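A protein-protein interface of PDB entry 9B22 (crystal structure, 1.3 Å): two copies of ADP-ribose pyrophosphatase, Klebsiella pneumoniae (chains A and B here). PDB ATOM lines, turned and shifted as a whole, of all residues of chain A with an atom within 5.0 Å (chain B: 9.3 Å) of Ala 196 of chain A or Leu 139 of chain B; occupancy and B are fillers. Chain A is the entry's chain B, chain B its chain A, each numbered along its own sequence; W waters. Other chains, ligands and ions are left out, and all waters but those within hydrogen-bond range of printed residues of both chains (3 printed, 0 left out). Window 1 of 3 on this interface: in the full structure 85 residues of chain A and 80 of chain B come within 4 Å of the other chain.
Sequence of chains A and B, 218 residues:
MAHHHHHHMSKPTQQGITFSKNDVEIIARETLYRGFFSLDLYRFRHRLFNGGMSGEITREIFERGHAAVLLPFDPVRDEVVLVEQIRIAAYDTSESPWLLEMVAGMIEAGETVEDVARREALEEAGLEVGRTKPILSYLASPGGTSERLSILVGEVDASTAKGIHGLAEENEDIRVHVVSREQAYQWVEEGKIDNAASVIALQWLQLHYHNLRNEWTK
N of Leu 139 of chain B lies within hydrogen-bond range of O of Asp 194 of chain A. The guanidinium group of Arg 148 of chain B is in hydrogen-bond range of the side-chain hydroxyl of Ser 94 of chain A (3.1 Å). The backbone carbonyl oxygen of Leu 139 of chain B sits at hydrogen-bond distance from the backbone NH of Ala 196 of chain A (2.9 Å). The side-chain amide nitrogen (NE2) of Gln 203 of chain B lies within hydrogen-bond range of the backbone carbonyl oxygen (O) of Ile 200 of chain A (3.1 Å). OD2 of Asp 194 of chain A lies within salt-bridge range of NH2 of Arg 148 of chain B (2.8 Å). OG1 of Thr 93 of chain A is in hydrogen-bond range of NE of Arg 148 of chain B.
The backbone NH (N) of Leu 149 of chain B is in hydrogen-bond range of the backbone carbonyl oxygen (O) of Tyr 138 of chain B. The backbone carbonyl oxygen (O) of Glu 147 of chain B sits at hydrogen-bond distance from the backbone NH (N) of Ala 140 of chain B (3.0 Å). The side-chain hydroxyl of Ser 137 of chain B is in hydrogen-bond range of the side-chain hydroxyl of Ser 150 of chain B. The backbone carbonyl oxygen of Leu 136 of chain B is in hydrogen-bond range of the backbone NH of Ile 151 of chain B, at 2.8 Å. NH1 of Arg 148 of chain B sits at hydrogen-bond distance from OG of Ser 137 of chain B, 3.2 Å away. The side-chain amide oxygen (OD1) of Asn 195 of chain A sits at hydrogen-bond distance from the side-chain hydroxyl (OG) of Ser 198 of chain A.
Among the printed residues, pairs that only touch across the chains: Asp 194 of chain A with Tyr 138 of chain B, Asp 194 of chain A with Ser 137 of chain B, Ile 200 of chain A with Ile 200 of chain B, Thr 93 of chain A with His 66 of chain B, Ala 196 of chain A with Ala 140 of chain B, Leu 99 of chain A with Pro 142 of chain B, Ser 94 of chain A with Leu 139 of chain B, Tyr 138 of chain A with Ala 196 of chain B, Thr 93 of chain A with Leu 139 of chain B, Ala 90 of chain A with Leu 139 of chain B, Asn 195 of chain A with Leu 139 of chain B, Ala 196 of chain A with Tyr 138 of chain B, Ile 200 of chain A with Val 199 of chain B, Val 199 of chain A with Ile 200 of chain B, Leu 99 of chain A with Leu 139 of chain B and Val 199 of chain A with Leu 136 of chain B.
Of chain B, only Tyr 138 (3.8 Å), Leu 139 (2.9 Å) and Ala 140 (3.6 Å) come within 4 Å of Ala 196 of chain A. Of chain A, only Ala 90 (3.7 Å), Thr 93 (3.7 Å), Ser 94 (3.6 Å), Leu 99 (3.9 Å), Asp 194 (2.8 Å), Asn 195 (3.8 Å) and Ala 196 (2.9 Å) come within 4 Å of Leu 139 of chain B. Ala 90 of chain A touches one residue of chain B. Of the printed residues of chain A, Ser 137 of chain B touches Asp 194. Of the printed residues of chain A, Gln 203 of chain B touches Ile 200 (3.1 Å). Printed residues of chain B within 4 Å of Asp 194 of chain A: Ser 137 (3.4 Å), Tyr 138 (3.1 Å), Leu 139 (2.8 Å) and Arg 148 (2.8 Å). Of the printed residues of chain A, Leu 136 of chain B touches Val 199 (3.99 Å). Printed residues of chain A within 4 Å of Ala 140 of chain B: Ala 196. The nearest residue of chain B that does not touch Ala 196 of chain A is Ile 200 of chain B (4.2 Å).
Of the 13 printed residues of chain A, 10 touch a printed residue of chain B. Hydrophobic or aromatic side chains of chain A within 4 Å of the printed part of chain B: Ala 90, Leu 99, Tyr 138, Ala 196, Val 199 and Ile 200. Hydrophobic or aromatic side chains of chain B that line the printed part of chain A: His 66, Leu 136, Tyr 138, Leu 139, Pro 142, Ala 196, Val 199 and Ile 200. Among the printed residues, Asp or Glu carboxylates within 4 Å of a Lys or Arg side-chain nitrogen of the other chain: Asp 194 of chain A with Arg 148 of chain B (2.8 Å).
Tyr 138 of chain A touches Ala 196 of chain B, and with the chains exchanged Ala 196 of chain A touches Tyr 138 of chain B. Val 199 of chain A touches Ile 200 of chain B, and with the chains exchanged Ile 200 of chain A touches Val 199 of chain B. Ile 200 of chain B touches its own counterpart, Ile 200 of chain A.
Water W2 lies within hydrogen-bond range of the backbone carbonyl oxygen of Ala 140 of chain B (2.7 Å) and the side-chain hydroxyl of Tyr 138 of chain A (2.8 Å). Water W1 lies within hydrogen-bond range of the side-chain carboxylate (OD1) of Asp 194 of chain A, the side-chain hydroxyl (OG) of Ser 94 of chain A and the guanidinium group (NH2) of Arg 148 of chain B. Water W3 bridges the backbone carbonyl oxygen (O) of Ser 146 of chain B and the side-chain hydroxyl (OG1) of Thr 93 of chain A.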
ATOM      1  N   ALA A  90     -23.888 -26.851  25.008  1.00  0.00           N
ATOM      2  CA  ALA A  90     -24.791 -25.793  25.440  1.00  0.00           C
ATOM      3  C   ALA A  90     -25.814 -26.271  26.459  1.00  0.00           C
ATOM      4  O   ALA A  90     -26.454 -25.436  27.103  1.00  0.00           O
ATOM      5  CB  ALA A  90     -25.549 -25.245  24.224  1.00  0.00           C
ATOM      6  N   THR A  93     -26.622 -24.884  30.318  1.00  0.00           N
ATOM      7  CA  THR A  93     -26.941 -23.492  30.594  1.00  0.00           C
ATOM      8  C   THR A  93     -27.936 -22.895  29.605  1.00  0.00           C
ATOM      9  O   THR A  93     -28.147 -21.681  29.635  1.00  0.00           O
ATOM     10  CB  THR A  93     -25.697 -22.588  30.609  1.00  0.00           C
ATOM     11  OG1 THR A  93     -25.180 -22.461  29.279  1.00  0.00           O
ATOM     12  CG2 THR A  93     -24.593 -23.098  31.537  1.00  0.00           C
ATOM     13  N   SER A  94     -28.544 -23.701  28.730  1.00  0.00           N
ATOM     14  CA  SER A  94     -29.376 -23.187  27.655  1.00  0.00           C
ATOM     15  C   SER A  94     -30.753 -23.838  27.641  1.00  0.00           C
ATOM     16  O   SER A  94     -30.961 -24.934  28.170  1.00  0.00           O
ATOM     17  CB  SER A  94     -28.720 -23.458  26.309  1.00  0.00           C
ATOM     18  OG  SER A  94     -27.388 -22.972  26.295  1.00  0.00           O
ATOM     19  N   LEU A  99     -29.151 -25.118  18.604  1.00  0.00           N
ATOM     20  CA  LEU A  99     -28.938 -23.685  18.512  1.00  0.00           C
ATOM     21  C   LEU A  99     -29.169 -23.205  17.093  1.00  0.00           C
ATOM     22  O   LEU A  99     -28.959 -23.944  16.134  1.00  0.00           O
ATOM     23  CB  LEU A  99     -27.495 -23.327  18.880  1.00  0.00           C
ATOM     24  CG  LEU A  99     -27.010 -23.800  20.256  1.00  0.00           C
ATOM     25  CD1 LEU A  99     -25.639 -23.218  20.557  1.00  0.00           C
ATOM     26  CD2 LEU A  99     -27.957 -23.425  21.372  1.00  0.00           C
ATOM     27  N   TYR A 138     -12.220 -13.180  15.585  1.00  0.00           N
ATOM     28  CA  TYR A 138     -12.195 -13.024  17.031  1.00  0.00           C
ATOM     29  C   TYR A 138     -11.686 -14.285  17.711  1.00  0.00           C
ATOM     30  O   TYR A 138     -11.804 -15.400  17.186  1.00  0.00           O
ATOM     31  CB  TYR A 138     -13.589 -12.664  17.621  1.00  0.00           C
ATOM     32  CG  TYR A 138     -14.605 -13.775  17.524  1.00  0.00           C
ATOM     33  CD1 TYR A 138     -15.316 -13.990  16.354  1.00  0.00           C
ATOM     34  CD2 TYR A 138     -14.899 -14.580  18.606  1.00  0.00           C
ATOM     35  CE1 TYR A 138     -16.236 -14.990  16.256  1.00  0.00           C
ATOM     36  CE2 TYR A 138     -15.830 -15.588  18.514  1.00  0.00           C
ATOM     37  CZ  TYR A 138     -16.501 -15.793  17.333  1.00  0.00           C
ATOM     38  OH  TYR A 138     -17.423 -16.804  17.222  1.00  0.00           O
ATOM     39  N   ASP A 194     -27.788 -16.831  21.056  1.00  0.00           N
ATOM     40  CA  ASP A 194     -26.851 -16.457  22.106  1.00  0.00           C
ATOM     41  C   ASP A 194     -25.536 -17.225  22.006  1.00  0.00           C
ATOM     42  O   ASP A 194     -24.831 -17.361  23.000  1.00  0.00           O
ATOM     43  CB  ASP A 194     -27.467 -16.595  23.521  1.00  0.00           C
ATOM     44  CG  ASP A 194     -27.691 -18.032  23.945  1.00  0.00           C
ATOM     45  OD1 ASP A 194     -27.592 -18.963  23.115  1.00  0.00           O
ATOM     46  OD2 ASP A 194     -27.981 -18.225  25.146  1.00  0.00           O
ATOM     47  N   ASN A 195     -25.170 -17.682  20.809  1.00  0.00           N
ATOM     48  CA  ASN A 195     -23.820 -18.193  20.574  1.00  0.00           C
ATOM     49  C   ASN A 195     -22.968 -17.066  19.989  1.00  0.00           C
ATOM     50  O   ASN A 195     -23.458 -16.250  19.207  1.00  0.00           O
ATOM     51  CB  ASN A 195     -23.830 -19.403  19.627  1.00  0.00           C
ATOM     52  CG  ASN A 195     -24.518 -19.129  18.300  1.00  0.00           C
ATOM     53  OD1 ASN A 195     -23.854 -18.830  17.303  1.00  0.00           O
ATOM     54  ND2 ASN A 195     -25.835 -19.257  18.270  1.00  0.00           N
ATOM     55  N   ALA A 196     -21.704 -16.996  20.434  1.00  0.00           N
ATOM     56  CA  ALA A 196     -20.853 -15.848  20.119  1.00  0.00           C
ATOM     57  C   ALA A 196     -20.826 -15.496  18.636  1.00  0.00           C
ATOM     58  O   ALA A 196     -20.960 -14.328  18.264  1.00  0.00           O
ATOM     59  CB  ALA A 196     -19.435 -16.139  20.608  1.00  0.00           C
ATOM     60  N   ALA A 197     -20.632 -16.488  17.766  1.00  0.00           N
ATOM     61  CA  ALA A 197     -20.445 -16.165  16.361  1.00  0.00           C
ATOM     62  C   ALA A 197     -21.684 -15.496  15.783  1.00  0.00           C
ATOM     63  O   ALA A 197     -21.578 -14.552  14.997  1.00  0.00           O
ATOM     64  CB  ALA A 197     -20.150 -17.432  15.560  1.00  0.00           C
ATOM     65  N   SER A 198     -22.869 -15.969  16.162  1.00  0.00           N
ATOM     66  CA  SER A 198     -24.098 -15.393  15.633  1.00  0.00           C
ATOM     67  C   SER A 198     -24.384 -14.031  16.246  1.00  0.00           C
ATOM     68  O   SER A 198     -24.869 -13.131  15.561  1.00  0.00           O
ATOM     69  CB  SER A 198     -25.276 -16.324  15.896  1.00  0.00           C
ATOM     70  OG  SER A 198     -25.098 -17.557  15.237  1.00  0.00           O
ATOM     71  N   VAL A 199     -24.122 -13.866  17.544  1.00  0.00           N
ATOM     72  CA  VAL A 199     -24.293 -12.566  18.189  1.00  0.00           C
ATOM     73  C   VAL A 199     -23.406 -11.538  17.511  1.00  0.00           C
ATOM     74  O   VAL A 199     -23.841 -10.433  17.169  1.00  0.00           O
ATOM     75  CB  VAL A 199     -23.998 -12.675  19.695  1.00  0.00           C
ATOM     76  CG1 VAL A 199     -24.013 -11.304  20.365  1.00  0.00           C
ATOM     77  CG2 VAL A 199     -25.031 -13.578  20.387  1.00  0.00           C
ATOM     78  N   ILE A 200     -22.136 -11.882  17.330  1.00  0.00           N
ATOM     79  CA  ILE A 200     -21.204 -10.941  16.721  1.00  0.00           C
ATOM     80  C   ILE A 200     -21.633 -10.616  15.297  1.00  0.00           C
ATOM     81  O   ILE A 200     -21.656  -9.454  14.880  1.00  0.00           O
ATOM     82  CB  ILE A 200     -19.771 -11.502  16.793  1.00  0.00           C
ATOM     83  CG1 ILE A 200     -19.280 -11.523  18.247  1.00  0.00           C
ATOM     84  CG2 ILE A 200     -18.854 -10.677  15.922  1.00  0.00           C
ATOM     85  CD1 ILE A 200     -18.006 -12.289  18.437  1.00  0.00           C
ATOM     86  N   ALA A 201     -21.994 -11.640  14.528  1.00  0.00           N
ATOM     87  CA  ALA A 201     -22.336 -11.409  13.124  1.00  0.00           C
ATOM     88  C   ALA A 201     -23.608 -10.576  12.985  1.00  0.00           C
ATOM     89  O   ALA A 201     -23.682  -9.665  12.153  1.00  0.00           O
ATOM     90  CB  ALA A 201     -22.486 -12.745  12.401  1.00  0.00           C
ATOM     91  N   GLY B  65     -16.393 -23.899  33.829  1.00  0.00           N
ATOM     92  CA  GLY B  65     -17.310 -23.010  34.506  1.00  0.00           C
ATOM     93  C   GLY B  65     -17.661 -21.838  33.598  1.00  0.00           C
ATOM     94  O   GLY B  65     -17.386 -21.828  32.397  1.00  0.00           O
ATOM     95  N   HIS B  66     -18.215 -20.806  34.227  1.00  0.00           N
ATOM     96  CA  HIS B  66     -18.801 -19.661  33.546  1.00  0.00           C
ATOM     97  C   HIS B  66     -18.224 -18.373  34.101  1.00  0.00           C
ATOM     98  O   HIS B  66     -17.574 -18.356  35.145  1.00  0.00           O
ATOM     99  CB  HIS B  66     -20.328 -19.728  33.686  1.00  0.00           C
ATOM    100  CG  HIS B  66     -20.848 -21.058  33.271  1.00  0.00           C
ATOM    101  ND1 HIS B  66     -20.703 -21.531  31.985  1.00  0.00           N
ATOM    102  CD2 HIS B  66     -21.352 -22.082  33.995  1.00  0.00           C
ATOM    103  CE1 HIS B  66     -21.158 -22.765  31.920  1.00  0.00           C
ATOM    104  NE2 HIS B  66     -21.584 -23.117  33.122  1.00  0.00           N
ATOM    105  N   LEU B 136     -25.943  -8.901  27.618  1.00  0.00           N
ATOM    106  CA  LEU B 136     -26.197 -10.135  26.886  1.00  0.00           C
ATOM    107  C   LEU B 136     -25.442 -11.239  27.611  1.00  0.00           C
ATOM    108  O   LEU B 136     -24.447 -10.986  28.282  1.00  0.00           O
ATOM    109  CB  LEU B 136     -25.671 -10.067  25.434  1.00  0.00           C
ATOM    110  CG  LEU B 136     -26.292  -9.060  24.461  1.00  0.00           C
ATOM    111  CD1 LEU B 136     -25.406  -8.903  23.236  1.00  0.00           C
ATOM    112  CD2 LEU B 136     -27.711  -9.468  24.043  1.00  0.00           C
ATOM    113  N   SER B 137     -25.913 -12.468  27.448  1.00  0.00           N
ATOM    114  CA  SER B 137     -25.226 -13.651  27.935  1.00  0.00           C
ATOM    115  C   SER B 137     -25.050 -14.588  26.749  1.00  0.00           C
ATOM    116  O   SER B 137     -26.001 -14.819  25.992  1.00  0.00           O
ATOM    117  CB  SER B 137     -26.031 -14.316  29.036  1.00  0.00           C
ATOM    118  OG  SER B 137     -25.393 -15.499  29.431  1.00  0.00           O
ATOM    119  N   TYR B 138     -23.839 -15.092  26.553  1.00  0.00           N
ATOM    120  CA  TYR B 138     -23.525 -15.843  25.345  1.00  0.00           C
ATOM    121  C   TYR B 138     -22.677 -17.074  25.649  1.00  0.00           C
ATOM    122  O   TYR B 138     -21.934 -17.138  26.635  1.00  0.00           O
ATOM    123  CB  TYR B 138     -22.830 -14.968  24.274  1.00  0.00           C
ATOM    124  CG  TYR B 138     -21.424 -14.559  24.633  1.00  0.00           C
ATOM    125  CD1 TYR B 138     -21.181 -13.436  25.427  1.00  0.00           C
ATOM    126  CD2 TYR B 138     -20.322 -15.289  24.185  1.00  0.00           C
ATOM    127  CE1 TYR B 138     -19.906 -13.063  25.776  1.00  0.00           C
ATOM    128  CE2 TYR B 138     -19.037 -14.912  24.525  1.00  0.00           C
ATOM    129  CZ  TYR B 138     -18.841 -13.800  25.315  1.00  0.00           C
ATOM    130  OH  TYR B 138     -17.584 -13.445  25.694  1.00  0.00           O
ATOM    131  N   LEU B 139     -22.773 -18.045  24.745  1.00  0.00           N
ATOM    132  CA  LEU B 139     -21.924 -19.234  24.751  1.00  0.00           C
ATOM    133  C   LEU B 139     -20.680 -18.947  23.917  1.00  0.00           C
ATOM    134  O   LEU B 139     -20.782 -18.570  22.747  1.00  0.00           O
ATOM    135  CB  LEU B 139     -22.694 -20.402  24.139  1.00  0.00           C
ATOM    136  CG  LEU B 139     -23.894 -20.886  24.968  1.00  0.00           C
ATOM    137  CD1 LEU B 139     -24.886 -21.584  24.054  1.00  0.00           C
ATOM    138  CD2 LEU B 139     -23.464 -21.805  26.070  1.00  0.00           C
ATOM    139  N   ALA B 140     -19.500 -19.117  24.525  1.00  0.00           N
ATOM    140  CA  ALA B 140     -18.255 -18.750  23.850  1.00  0.00           C
ATOM    141  C   ALA B 140     -18.031 -19.550  22.568  1.00  0.00           C
ATOM    142  O   ALA B 140     -17.557 -19.000  21.569  1.00  0.00           O
ATOM    143  CB  ALA B 140     -17.073 -18.959  24.793  1.00  0.00           C
ATOM    144  N   SER B 141     -18.264 -20.866  22.605  1.00  0.00           N
ATOM    145  CA  SER B 141     -17.949 -21.732  21.478  1.00  0.00           C
ATOM    146  C   SER B 141     -18.584 -23.090  21.727  1.00  0.00           C
ATOM    147  O   SER B 141     -17.905 -24.051  22.119  1.00  0.00           O
ATOM    148  CB  SER B 141     -16.441 -21.877  21.318  1.00  0.00           C
ATOM    149  OG  SER B 141     -16.166 -22.652  20.166  1.00  0.00           O
ATOM    150  N   PRO B 142     -19.893 -23.202  21.507  1.00  0.00           N
ATOM    151  CA  PRO B 142     -20.644 -24.320  22.087  1.00  0.00           C
ATOM    152  C   PRO B 142     -20.501 -25.651  21.363  1.00  0.00           C
ATOM    153  O   PRO B 142     -21.084 -26.631  21.827  1.00  0.00           O
ATOM    154  CB  PRO B 142     -22.094 -23.811  22.056  1.00  0.00           C
ATOM    155  CG  PRO B 142     -22.125 -22.808  20.949  1.00  0.00           C
ATOM    156  CD  PRO B 142     -20.774 -22.128  21.025  1.00  0.00           C
ATOM    157  N   GLY B 143     -19.715 -25.722  20.285  1.00  0.00           N
ATOM    158  CA  GLY B 143     -19.362 -27.008  19.729  1.00  0.00           C
ATOM    159  C   GLY B 143     -18.333 -27.755  20.551  1.00  0.00           C
ATOM    160  O   GLY B 143     -18.230 -28.974  20.430  1.00  0.00           O
ATOM    161  N   GLY B 144     -17.572 -27.057  21.388  1.00  0.00           N
ATOM    162  CA  GLY B 144     -16.526 -27.711  22.153  1.00  0.00           C
ATOM    163  C   GLY B 144     -16.356 -27.301  23.600  1.00  0.00           C
ATOM    164  O   GLY B 144     -15.578 -27.948  24.296  1.00  0.00           O
ATOM    165  N   THR B 145     -17.012 -26.242  24.065  1.00  0.00           N
ATOM    166  CA  THR B 145     -16.916 -25.831  25.467  1.00  0.00           C
ATOM    167  C   THR B 145     -18.298 -25.445  25.963  1.00  0.00           C
ATOM    168  O   THR B 145     -19.101 -24.891  25.216  1.00  0.00           O
ATOM    169  CB  THR B 145     -15.916 -24.667  25.660  1.00  0.00           C
ATOM    170  OG1 THR B 145     -15.838 -24.292  27.039  1.00  0.00           O
ATOM    171  CG2 THR B 145     -16.300 -23.445  24.880  1.00  0.00           C
ATOM    172  N   SER B 146     -18.562 -25.716  27.242  1.00  0.00           N
ATOM    173  CA  SER B 146     -19.822 -25.325  27.847  1.00  0.00           C
ATOM    174  C   SER B 146     -19.832 -23.877  28.302  1.00  0.00           C
ATOM    175  O   SER B 146     -20.874 -23.405  28.769  1.00  0.00           O
ATOM    176  CB  SER B 146     -20.098 -26.200  29.050  1.00  0.00           C
ATOM    177  OG  SER B 146     -19.038 -26.036  29.958  1.00  0.00           O
ATOM    178  N   GLU B 147     -18.711 -23.164  28.172  1.00  0.00           N
ATOM    179  CA  GLU B 147     -18.586 -21.861  28.815  1.00  0.00           C
ATOM    180  C   GLU B 147     -19.634 -20.860  28.342  1.00  0.00           C
ATOM    181  O   GLU B 147     -19.775 -20.579  27.138  1.00  0.00           O
ATOM    182  CB  GLU B 147     -17.209 -21.258  28.576  1.00  0.00           C
ATOM    183  CG  GLU B 147     -16.980 -20.020  29.411  1.00  0.00           C
ATOM    184  CD  GLU B 147     -15.709 -19.272  29.082  1.00  0.00           C
ATOM    185  OE1 GLU B 147     -15.178 -19.416  27.969  1.00  0.00           O
ATOM    186  OE2 GLU B 147     -15.229 -18.538  29.975  1.00  0.00           O
ATOM    187  N   ARG B 148     -20.297 -20.255  29.324  1.00  0.00           N
ATOM    188  CA  ARG B 148     -21.197 -19.127  29.127  1.00  0.00           C
ATOM    189  C   ARG B 148     -20.621 -17.914  29.843  1.00  0.00           C
ATOM    190  O   ARG B 148     -20.037 -18.033  30.923  1.00  0.00           O
ATOM    191  CB  ARG B 148     -22.592 -19.440  29.688  1.00  0.00           C
ATOM    192  CG  ARG B 148     -23.580 -18.299  29.604  1.00  0.00           C
ATOM    193  CD  ARG B 148     -25.004 -18.773  29.910  1.00  0.00           C
ATOM    194  NE  ARG B 148     -25.571 -19.639  28.885  1.00  0.00           N
ATOM    195  CZ  ARG B 148     -26.189 -19.179  27.802  1.00  0.00           C
ATOM    196  NH1 ARG B 148     -26.264 -17.882  27.550  1.00  0.00           N
ATOM    197  NH2 ARG B 148     -26.742 -20.038  26.945  1.00  0.00           N
ATOM    198  N   LEU B 149     -20.743 -16.752  29.209  1.00  0.00           N
ATOM    199  CA  LEU B 149     -20.300 -15.493  29.788  1.00  0.00           C
ATOM    200  C   LEU B 149     -21.467 -14.524  29.810  1.00  0.00           C
ATOM    201  O   LEU B 149     -22.231 -14.440  28.851  1.00  0.00           O
ATOM    202  CB  LEU B 149     -19.150 -14.874  28.973  1.00  0.00           C
ATOM    203  CG  LEU B 149     -17.874 -15.702  28.953  1.00  0.00           C
ATOM    204  CD1 LEU B 149     -17.823 -16.622  27.737  1.00  0.00           C
ATOM    205  CD2 LEU B 149     -16.657 -14.792  28.992  1.00  0.00           C
ATOM    206  N   SER B 150     -21.628 -13.819  30.923  1.00  0.00           N
ATOM    207  CA  SER B 150     -22.727 -12.882  31.092  1.00  0.00           C
ATOM    208  C   SER B 150     -22.151 -11.492  31.258  1.00  0.00           C
ATOM    209  O   SER B 150     -21.306 -11.267  32.130  1.00  0.00           O
ATOM    210  CB  SER B 150     -23.543 -13.279  32.311  1.00  0.00           C
ATOM    211  OG  SER B 150     -24.095 -14.566  32.077  1.00  0.00           O
ATOM    212  N   ILE B 151     -22.568 -10.582  30.384  1.00  0.00           N
ATOM    213  CA  ILE B 151     -21.997  -9.250  30.302  1.00  0.00           C
ATOM    214  C   ILE B 151     -22.933  -8.251  30.945  1.00  0.00           C
ATOM    215  O   ILE B 151     -24.135  -8.233  30.644  1.00  0.00           O
ATOM    216  CB  ILE B 151     -21.749  -8.826  28.841  1.00  0.00           C
ATOM    217  CG1 ILE B 151     -21.059  -9.918  28.021  1.00  0.00           C
ATOM    218  CG2 ILE B 151     -20.958  -7.534  28.818  1.00  0.00           C
ATOM    219  CD1 ILE B 151     -20.928  -9.543  26.552  1.00  0.00           C
ATOM    220  N   ASN B 195     -11.294 -10.037  20.914  1.00  0.00           N
ATOM    221  CA  ASN B 195     -11.755 -11.097  21.794  1.00  0.00           C
ATOM    222  C   ASN B 195     -13.270 -10.986  21.901  1.00  0.00           C
ATOM    223  O   ASN B 195     -13.818  -9.886  21.933  1.00  0.00           O
ATOM    224  CB  ASN B 195     -11.070 -11.034  23.165  1.00  0.00           C
ATOM    225  CG  ASN B 195     -11.246  -9.703  23.857  1.00  0.00           C
ATOM    226  OD1 ASN B 195     -12.146  -9.543  24.682  1.00  0.00           O
ATOM    227  ND2 ASN B 195     -10.382  -8.730  23.529  1.00  0.00           N
ATOM    228  N   ALA B 196     -13.941 -12.138  21.969  1.00  0.00           N
ATOM    229  CA  ALA B 196     -15.397 -12.160  21.845  1.00  0.00           C
ATOM    230  C   ALA B 196     -16.090 -11.241  22.846  1.00  0.00           C
ATOM    231  O   ALA B 196     -17.037 -10.534  22.493  1.00  0.00           O
ATOM    232  CB  ALA B 196     -15.921 -13.593  22.014  1.00  0.00           C
ATOM    233  N   ALA B 197     -15.674 -11.272  24.119  1.00  0.00           N
ATOM    234  CA  ALA B 197     -16.404 -10.518  25.136  1.00  0.00           C
ATOM    235  C   ALA B 197     -16.369  -9.028  24.830  1.00  0.00           C
ATOM    236  O   ALA B 197     -17.375  -8.329  24.959  1.00  0.00           O
ATOM    237  CB  ALA B 197     -15.804 -10.778  26.515  1.00  0.00           C
ATOM    238  N   VAL B 199     -15.715  -7.617  21.824  1.00  0.00           N
ATOM    239  CA  VAL B 199     -16.419  -7.366  20.568  1.00  0.00           C
ATOM    240  C   VAL B 199     -17.915  -7.272  20.809  1.00  0.00           C
ATOM    241  O   VAL B 199     -18.568  -6.317  20.391  1.00  0.00           O
ATOM    242  CB  VAL B 199     -16.070  -8.439  19.522  1.00  0.00           C
ATOM    243  CG1 VAL B 199     -16.977  -8.326  18.300  1.00  0.00           C
ATOM    244  CG2 VAL B 199     -14.611  -8.334  19.120  1.00  0.00           C
ATOM    245  N   ILE B 200     -18.463  -8.249  21.528  1.00  0.00           N
ATOM    246  CA  ILE B 200     -19.904  -8.273  21.772  1.00  0.00           C
ATOM    247  C   ILE B 200     -20.332  -7.069  22.600  1.00  0.00           C
ATOM    248  O   ILE B 200     -21.327  -6.397  22.292  1.00  0.00           O
ATOM    249  CB  ILE B 200     -20.307  -9.600  22.440  1.00  0.00           C
ATOM    250  CG1 ILE B 200     -20.137 -10.748  21.441  1.00  0.00           C
ATOM    251  CG2 ILE B 200     -21.729  -9.536  22.961  1.00  0.00           C
ATOM    252  CD1 ILE B 200     -20.264 -12.138  22.043  1.00  0.00           C
ATOM    253  N   GLN B 203     -19.923  -3.769  20.434  1.00  0.00           N
ATOM    254  CA  GLN B 203     -20.989  -3.693  19.439  1.00  0.00           C
ATOM    255  C   GLN B 203     -22.317  -3.334  20.092  1.00  0.00           C
ATOM    256  O   GLN B 203     -23.077  -2.507  19.565  1.00  0.00           O
ATOM    257  CB  GLN B 203     -21.133  -5.023  18.716  1.00  0.00           C
ATOM    258  CG  GLN B 203     -20.059  -5.377  17.710  1.00  0.00           C
ATOM    259  CD  GLN B 203     -20.351  -6.753  17.151  1.00  0.00           C
ATOM    260  OE1 GLN B 203     -20.834  -7.635  17.874  1.00  0.00           O
ATOM    261  NE2 GLN B 203     -20.084  -6.942  15.891  1.00  0.00           N
HETATM  262  O   HOH W   1     -28.763 -21.129  24.305  1.00  0.00           O
HETATM  263  O   HOH W   2     -17.658 -18.990  18.900  1.00  0.00           O
HETATM  264  O   HOH W   3     -23.415 -24.518  28.647  1.00  0.00           O
